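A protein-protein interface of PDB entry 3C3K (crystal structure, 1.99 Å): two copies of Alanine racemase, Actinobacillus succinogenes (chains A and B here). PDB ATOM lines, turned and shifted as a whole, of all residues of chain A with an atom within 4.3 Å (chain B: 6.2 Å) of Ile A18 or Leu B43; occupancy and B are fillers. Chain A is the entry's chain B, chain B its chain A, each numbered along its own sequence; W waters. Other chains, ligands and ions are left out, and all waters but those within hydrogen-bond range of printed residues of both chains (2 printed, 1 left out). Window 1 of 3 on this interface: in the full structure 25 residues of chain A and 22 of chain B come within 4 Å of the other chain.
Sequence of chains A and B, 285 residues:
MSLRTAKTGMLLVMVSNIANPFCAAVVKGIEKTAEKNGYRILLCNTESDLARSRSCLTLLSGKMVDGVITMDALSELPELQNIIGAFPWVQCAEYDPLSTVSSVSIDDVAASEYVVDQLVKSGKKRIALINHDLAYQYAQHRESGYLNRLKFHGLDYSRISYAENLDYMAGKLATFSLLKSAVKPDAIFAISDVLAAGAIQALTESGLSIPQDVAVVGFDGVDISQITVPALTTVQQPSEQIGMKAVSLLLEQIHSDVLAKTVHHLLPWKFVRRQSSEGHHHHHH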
ATOM      1  N   VAL A  15     -13.732  -1.159  11.525  1.00  0.00           N
ATOM      2  CA  VAL A  15     -12.361  -0.876  11.123  1.00  0.00           C
ATOM      3  C   VAL A  15     -11.960   0.544  11.530  1.00  0.00           C
ATOM      4  O   VAL A  15     -12.751   1.498  11.372  1.00  0.00           O
ATOM      5  CB  VAL A  15     -12.294  -1.011   9.598  1.00  0.00           C
ATOM      6  CG1 VAL A  15     -10.946  -0.635   9.045  1.00  0.00           C
ATOM      7  CG2 VAL A  15     -12.572  -2.475   9.252  1.00  0.00           C
ATOM      8  N   ASN A  17      -9.428   2.408  10.204  1.00  0.00           N
ATOM      9  CA  ASN A  17      -9.245   3.232   8.978  1.00  0.00           C
ATOM     10  C   ASN A  17      -8.991   2.324   7.797  1.00  0.00           C
ATOM     11  O   ASN A  17      -7.974   1.653   7.682  1.00  0.00           O
ATOM     12  CB  ASN A  17      -8.064   4.243   9.158  1.00  0.00           C
ATOM     13  CG  ASN A  17      -7.864   5.160   7.961  1.00  0.00           C
ATOM     14  OD1 ASN A  17      -8.330   4.886   6.861  1.00  0.00           O
ATOM     15  ND2 ASN A  17      -7.127   6.261   8.176  1.00  0.00           N
ATOM     16  N   ILE A  18      -9.931   2.311   6.904  1.00  0.00           N
ATOM     17  CA  ILE A  18      -9.908   1.400   5.806  1.00  0.00           C
ATOM     18  C   ILE A  18      -8.726   1.704   4.842  1.00  0.00           C
ATOM     19  O   ILE A  18      -8.283   0.813   4.102  1.00  0.00           O
ATOM     20  CB  ILE A  18     -11.314   1.398   5.134  1.00  0.00           C
ATOM     21  CG1 ILE A  18     -11.642  -0.018   4.674  1.00  0.00           C
ATOM     22  CG2 ILE A  18     -11.516   2.617   4.139  1.00  0.00           C
ATOM     23  CD1 ILE A  18     -12.856  -0.088   3.809  1.00  0.00           C
ATOM     24  N   ALA A  19      -8.205   2.925   4.879  1.00  0.00           N
ATOM     25  CA  ALA A  19      -7.007   3.280   4.129  1.00  0.00           C
ATOM     26  C   ALA A  19      -5.683   2.934   4.782  1.00  0.00           C
ATOM     27  O   ALA A  19      -4.650   3.006   4.119  1.00  0.00           O
ATOM     28  CB  ALA A  19      -6.979   4.736   3.665  1.00  0.00           C
ATOM     29  N   ASN A  20      -5.717   2.501   6.036  1.00  0.00           N
ATOM     30  CA  ASN A  20      -4.518   2.037   6.740  1.00  0.00           C
ATOM     31  C   ASN A  20      -4.183   0.610   6.319  1.00  0.00           C
ATOM     32  O   ASN A  20      -4.960  -0.286   6.526  1.00  0.00           O
ATOM     33  CB  ASN A  20      -4.778   2.105   8.226  1.00  0.00           C
ATOM     34  CG  ASN A  20      -3.558   1.779   9.045  1.00  0.00           C
ATOM     35  OD1 ASN A  20      -2.490   1.501   8.509  1.00  0.00           O
ATOM     36  ND2 ASN A  20      -3.710   1.838  10.377  1.00  0.00           N
ATOM     37  N   LEU A  42     -18.890  -8.356   7.049  1.00  0.00           N
ATOM     38  CA  LEU A  42     -19.301  -7.009   6.664  1.00  0.00           C
ATOM     39  C   LEU A  42     -18.388  -6.029   7.370  1.00  0.00           C
ATOM     40  O   LEU A  42     -18.076  -6.216   8.580  1.00  0.00           O
ATOM     41  CB  LEU A  42     -20.729  -6.736   7.043  1.00  0.00           C
ATOM     42  CG  LEU A  42     -21.890  -7.235   6.205  1.00  0.00           C
ATOM     43  CD1 LEU A  42     -23.150  -6.839   6.951  1.00  0.00           C
ATOM     44  CD2 LEU A  42     -21.873  -6.676   4.788  1.00  0.00           C
ATOM     45  N   LEU A  43     -17.937  -4.998   6.666  1.00  0.00           N
ATOM     46  CA  LEU A  43     -17.063  -3.984   7.270  1.00  0.00           C
ATOM     47  C   LEU A  43     -17.781  -2.674   7.536  1.00  0.00           C
ATOM     48  O   LEU A  43     -18.694  -2.304   6.830  1.00  0.00           O
ATOM     49  CB  LEU A  43     -15.879  -3.652   6.335  1.00  0.00           C
ATOM     50  CG  LEU A  43     -15.020  -4.802   5.878  1.00  0.00           C
ATOM     51  CD1 LEU A  43     -14.043  -4.202   4.893  1.00  0.00           C
ATOM     52  CD2 LEU A  43     -14.274  -5.476   7.077  1.00  0.00           C
ATOM     53  N   ASN A  45     -16.352   1.328   8.212  1.00  0.00           N
ATOM     54  CA  ASN A  45     -15.192   2.175   8.391  1.00  0.00           C
ATOM     55  C   ASN A  45     -15.574   3.194   9.419  1.00  0.00           C
ATOM     56  O   ASN A  45     -15.955   4.332   9.095  1.00  0.00           O
ATOM     57  CB  ASN A  45     -14.778   2.874   7.076  1.00  0.00           C
ATOM     58  CG  ASN A  45     -13.491   3.615   7.234  1.00  0.00           C
ATOM     59  OD1 ASN A  45     -12.526   3.063   7.802  1.00  0.00           O
ATOM     60  ND2 ASN A  45     -13.466   4.895   6.798  1.00  0.00           N
ATOM     61  N   LEU B  11     -26.359   2.707   3.119  1.00  0.00           N
ATOM     62  CA  LEU B  11     -26.011   2.161   1.792  1.00  0.00           C
ATOM     63  C   LEU B  11     -25.010   0.991   1.827  1.00  0.00           C
ATOM     64  O   LEU B  11     -24.139   0.907   2.688  1.00  0.00           O
ATOM     65  CB  LEU B  11     -25.480   3.243   0.881  1.00  0.00           C
ATOM     66  CG  LEU B  11     -26.244   4.536   0.706  1.00  0.00           C
ATOM     67  CD1 LEU B  11     -25.346   5.423  -0.122  1.00  0.00           C
ATOM     68  CD2 LEU B  11     -27.662   4.338   0.031  1.00  0.00           C
ATOM     69  N   LEU B  12     -25.161   0.046   0.924  1.00  0.00           N
ATOM     70  CA  LEU B  12     -24.165  -1.003   0.839  1.00  0.00           C
ATOM     71  C   LEU B  12     -23.141  -0.672  -0.261  1.00  0.00           C
ATOM     72  O   LEU B  12     -23.520  -0.296  -1.370  1.00  0.00           O
ATOM     73  CB  LEU B  12     -24.838  -2.301   0.501  1.00  0.00           C
ATOM     74  CG  LEU B  12     -23.909  -3.468   0.247  1.00  0.00           C
ATOM     75  CD1 LEU B  12     -23.044  -3.821   1.481  1.00  0.00           C
ATOM     76  CD2 LEU B  12     -24.749  -4.683  -0.151  1.00  0.00           C
ATOM     77  N   VAL B  13     -21.854  -0.812   0.054  1.00  0.00           N
ATOM     78  CA  VAL B  13     -20.779  -0.663  -0.955  1.00  0.00           C
ATOM     79  C   VAL B  13     -20.042  -1.969  -1.171  1.00  0.00           C
ATOM     80  O   VAL B  13     -19.436  -2.487  -0.254  1.00  0.00           O
ATOM     81  CB  VAL B  13     -19.799   0.467  -0.623  1.00  0.00           C
ATOM     82  CG1 VAL B  13     -18.854   0.718  -1.789  1.00  0.00           C
ATOM     83  CG2 VAL B  13     -20.587   1.805  -0.348  1.00  0.00           C
ATOM     84  N   MET B  14     -20.108  -2.538  -2.371  1.00  0.00           N
ATOM     85  CA  MET B  14     -19.301  -3.707  -2.631  1.00  0.00           C
ATOM     86  C   MET B  14     -17.962  -3.257  -3.280  1.00  0.00           C
ATOM     87  O   MET B  14     -17.930  -2.750  -4.376  1.00  0.00           O
ATOM     88  CB  MET B  14     -20.072  -4.745  -3.479  1.00  0.00           C
ATOM     89  CG  MET B  14     -21.236  -5.460  -2.650  1.00  0.00           C
ATOM     90  SD  MET B  14     -22.681  -6.000  -3.616  1.00  0.00           S
ATOM     91  CE  MET B  14     -21.982  -7.337  -4.482  1.00  0.00           C
ATOM     92  N   VAL B  15     -16.853  -3.524  -2.606  1.00  0.00           N
ATOM     93  CA  VAL B  15     -15.551  -3.091  -3.024  1.00  0.00           C
ATOM     94  C   VAL B  15     -14.837  -4.277  -3.654  1.00  0.00           C
ATOM     95  O   VAL B  15     -14.958  -5.390  -3.178  1.00  0.00           O
ATOM     96  CB  VAL B  15     -14.829  -2.652  -1.742  1.00  0.00           C
ATOM     97  CG1 VAL B  15     -13.412  -2.233  -2.013  1.00  0.00           C
ATOM     98  CG2 VAL B  15     -15.610  -1.502  -1.082  1.00  0.00           C
ATOM     99  N   ILE B  18     -10.227  -3.888  -0.876  1.00  0.00           N
ATOM    100  CA  ILE B  18      -9.873  -2.850   0.097  1.00  0.00           C
ATOM    101  C   ILE B  18      -8.380  -2.608   0.271  1.00  0.00           C
ATOM    102  O   ILE B  18      -7.996  -1.501   0.674  1.00  0.00           O
ATOM    103  CB  ILE B  18     -10.466  -3.110   1.546  1.00  0.00           C
ATOM    104  CG1 ILE B  18      -9.924  -4.442   2.101  1.00  0.00           C
ATOM    105  CG2 ILE B  18     -11.947  -2.936   1.516  1.00  0.00           C
ATOM    106  CD1 ILE B  18     -10.422  -4.858   3.527  1.00  0.00           C
ATOM    107  N   ALA B  19      -7.546  -3.609  -0.063  1.00  0.00           N
ATOM    108  CA  ALA B  19      -6.115  -3.440  -0.047  1.00  0.00           C
ATOM    109  C   ALA B  19      -5.687  -2.729  -1.322  1.00  0.00           C
ATOM    110  O   ALA B  19      -4.545  -2.375  -1.442  1.00  0.00           O
ATOM    111  CB  ALA B  19      -5.386  -4.785   0.082  1.00  0.00           C
ATOM    112  N   ALA B  24      -9.719   2.349  -1.766  1.00  0.00           N
ATOM    113  CA  ALA B  24      -9.778   3.157  -0.570  1.00  0.00           C
ATOM    114  C   ALA B  24     -10.092   4.614  -0.927  1.00  0.00           C
ATOM    115  O   ALA B  24     -10.891   5.199  -0.253  1.00  0.00           O
ATOM    116  CB  ALA B  24      -8.542   3.050   0.294  1.00  0.00           C
ATOM    117  N   VAL B  27     -13.813   4.797  -1.990  1.00  0.00           N
ATOM    118  CA  VAL B  27     -14.664   4.617  -0.810  1.00  0.00           C
ATOM    119  C   VAL B  27     -14.702   5.905   0.042  1.00  0.00           C
ATOM    120  O   VAL B  27     -15.725   6.266   0.496  1.00  0.00           O
ATOM    121  CB  VAL B  27     -14.194   3.360  -0.001  1.00  0.00           C
ATOM    122  CG1 VAL B  27     -14.881   3.273   1.383  1.00  0.00           C
ATOM    123  CG2 VAL B  27     -14.449   2.088  -0.865  1.00  0.00           C
ATOM    124  N   LYS B  28     -13.585   6.596   0.202  1.00  0.00           N
ATOM    125  CA  LYS B  28     -13.526   7.868   0.890  1.00  0.00           C
ATOM    126  C   LYS B  28     -14.481   8.861   0.237  1.00  0.00           C
ATOM    127  O   LYS B  28     -15.254   9.504   0.910  1.00  0.00           O
ATOM    128  CB  LYS B  28     -12.079   8.402   0.879  1.00  0.00           C
ATOM    129  CG  LYS B  28     -12.017   9.942   1.038  1.00  0.00           C
ATOM    130  CD  LYS B  28     -11.384  10.355   2.317  1.00  0.00           C
ATOM    131  CE  LYS B  28      -9.888  10.613   2.104  1.00  0.00           C
ATOM    132  NZ  LYS B  28      -9.407  11.777   2.915  1.00  0.00           N
ATOM    133  N   GLU B  31     -18.095   7.699   1.006  1.00  0.00           N
ATOM    134  CA  GLU B  31     -18.479   7.981   2.398  1.00  0.00           C
ATOM    135  C   GLU B  31     -18.726   9.463   2.580  1.00  0.00           C
ATOM    136  O   GLU B  31     -19.609   9.836   3.320  1.00  0.00           O
ATOM    137  CB  GLU B  31     -17.358   7.782   3.382  1.00  0.00           C
ATOM    138  CG  GLU B  31     -17.027   6.482   3.848  1.00  0.00           C
ATOM    139  CD  GLU B  31     -15.799   6.615   4.785  1.00  0.00           C
ATOM    140  OE1 GLU B  31     -15.097   7.660   4.732  1.00  0.00           O
ATOM    141  OE2 GLU B  31     -15.559   5.724   5.592  1.00  0.00           O
ATOM    142  N   ILE B  41     -22.543   4.131   5.586  1.00  0.00           N
ATOM    143  CA  ILE B  41     -22.126   3.175   4.574  1.00  0.00           C
ATOM    144  C   ILE B  41     -21.672   1.842   5.221  1.00  0.00           C
ATOM    145  O   ILE B  41     -20.975   1.859   6.227  1.00  0.00           O
ATOM    146  CB  ILE B  41     -21.011   3.974   3.742  1.00  0.00           C
ATOM    147  CG1 ILE B  41     -21.663   4.982   2.758  1.00  0.00           C
ATOM    148  CG2 ILE B  41     -19.839   3.194   3.266  1.00  0.00           C
ATOM    149  CD1 ILE B  41     -22.536   4.429   1.749  1.00  0.00           C
ATOM    150  N   LEU B  42     -22.077   0.695   4.660  1.00  0.00           N
ATOM    151  CA  LEU B  42     -21.498  -0.591   5.025  1.00  0.00           C
ATOM    152  C   LEU B  42     -20.695  -1.166   3.844  1.00  0.00           C
ATOM    153  O   LEU B  42     -21.133  -1.010   2.717  1.00  0.00           O
ATOM    154  CB  LEU B  42     -22.618  -1.589   5.366  1.00  0.00           C
ATOM    155  CG  LEU B  42     -23.464  -1.114   6.541  1.00  0.00           C
ATOM    156  CD1 LEU B  42     -24.762  -1.944   6.543  1.00  0.00           C
ATOM    157  CD2 LEU B  42     -22.642  -1.327   7.840  1.00  0.00           C
ATOM    158  N   LEU B  43     -19.548  -1.807   4.088  1.00  0.00           N
ATOM    159  CA  LEU B  43     -18.722  -2.235   2.973  1.00  0.00           C
ATOM    160  C   LEU B  43     -18.652  -3.737   2.974  1.00  0.00           C
ATOM    161  O   LEU B  43     -18.632  -4.364   4.048  1.00  0.00           O
ATOM    162  CB  LEU B  43     -17.298  -1.729   3.098  1.00  0.00           C
ATOM    163  CG  LEU B  43     -17.104  -0.260   3.376  1.00  0.00           C
ATOM    164  CD1 LEU B  43     -15.675  -0.033   3.750  1.00  0.00           C
ATOM    165  CD2 LEU B  43     -17.415   0.597   2.200  1.00  0.00           C
ATOM    166  N   CYS B  44     -18.608  -4.312   1.787  1.00  0.00           N
ATOM    167  CA  CYS B  44     -18.267  -5.713   1.655  1.00  0.00           C
ATOM    168  C   CYS B  44     -16.979  -5.826   0.772  1.00  0.00           C
ATOM    169  O   CYS B  44     -16.985  -5.395  -0.355  1.00  0.00           O
ATOM    170  CB  CYS B  44     -19.449  -6.502   1.050  1.00  0.00           C
ATOM    171  SG  CYS B  44     -19.064  -8.328   1.111  1.00  0.00           S
ATOM    172  N   ASN B  45     -15.882  -6.397   1.280  1.00  0.00           N
ATOM    173  CA  ASN B  45     -14.743  -6.692   0.463  1.00  0.00           C
ATOM    174  C   ASN B  45     -15.024  -7.961  -0.389  1.00  0.00           C
ATOM    175  O   ASN B  45     -14.676  -9.080   0.002  1.00  0.00           O
ATOM    176  CB  ASN B  45     -13.513  -6.905   1.321  1.00  0.00           C
ATOM    177  CG  ASN B  45     -12.263  -6.956   0.502  1.00  0.00           C
ATOM    178  OD1 ASN B  45     -12.131  -6.209  -0.440  1.00  0.00           O
ATOM    179  ND2 ASN B  45     -11.369  -7.846   0.821  1.00  0.00           N
HETATM  180  O   HOH W   1     -17.997   2.243   6.376  1.00  0.00           O
HETATM  181  O   HOH W   2     -17.829   4.802   6.855  1.00  0.00           O
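The backbone carbonyl oxygen of Leu B43 sits at hydrogen-bond distance from the backbone NH of Leu A43 (2.8 Å). The side-chain carboxylate (OE2) of Glu B31 is in hydrogen-bond range of the side-chain amide nitrogen (ND2) of Asn A45 (2.6 Å).
OD1 of Asn B45 sits at hydrogen-bond distance from N of Ile B18 (3.0 Å). The backbone carbonyl oxygen (O) of Leu B11 lies within hydrogen-bond range of the backbone NH (N) of Leu B42 (2.9 Å). The side-chain amide oxygen (OD1) of Asn A45 sits at hydrogen-bond distance from the backbone NH (N) of Ile A18, 2.8 Å away. The backbone NH of Val B13 sits at hydrogen-bond distance from the backbone carbonyl oxygen of Leu B42.
Ile B18 touches Ile A18. Ile A18 touches Leu B43. Leu A42 touches Leu B43. Leu A43 touches Ile B18 (CD1 to CD1, 3.9 Å). Leu B42 touches Leu A43 (CA to O, 3.7 Å).
Ile A18 touches two residues of chain B. Printed residues of chain B within 4 Å of Leu A42: Leu B43 (3.7 Å). Of the printed residues of chain B, Leu A43 touches Ile B18 (3.9 Å), Leu B42 (3.7 Å) and Leu B43 (2.8 Å). Of the printed residues of chain A, Glu B31 touches Asn A45. Of chain A, only Ile A18, Leu A42 and Leu A43 come within 4 Å of Leu B43. The nearest printed residue of chain B that does not touch Ile A18 is Val B27 (4.4 Å). The nearest printed residue of chain A that does not touch Leu B43 is Asn A45 (4.5 Å). The nearest printed residue of chain A that does not touch Ile B18 is Ala A19 (6.0 Å).
Of the 16 printed residues of chain B, 4 touch a printed residue of chain A. Printed residues of chain B that touch a printed residue of chain A: Ile B18, Glu B31, Leu B42 and Leu B43. Hydrophobic or aromatic side chains of chain B that line the printed part of chain A: Ile B18 and Leu B43. Among the printed residues, 7 pairs touch across the chains.
Ile B18 touches its own counterpart, Ile A18. Ile A18 touches Leu B43, and with the chains exchanged Leu A43 touches Ile B18. Leu A42 touches Leu B43, and with the chains exchanged Leu A43 touches Leu B42. Leu B43 touches its own counterpart, Leu A43. Positions printed for both chains: 15, 18, 19, 42, 43 and 45.
Water W1 bridges N of Asn A45 (2.6 Å) and O of Ile B41 (3.0 Å). Water W2 bridges the side-chain carboxylate (OE2) of Glu B31 (2.8 Å) and the backbone carbonyl oxygen (O) of Asn A45 (3.0 Å).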
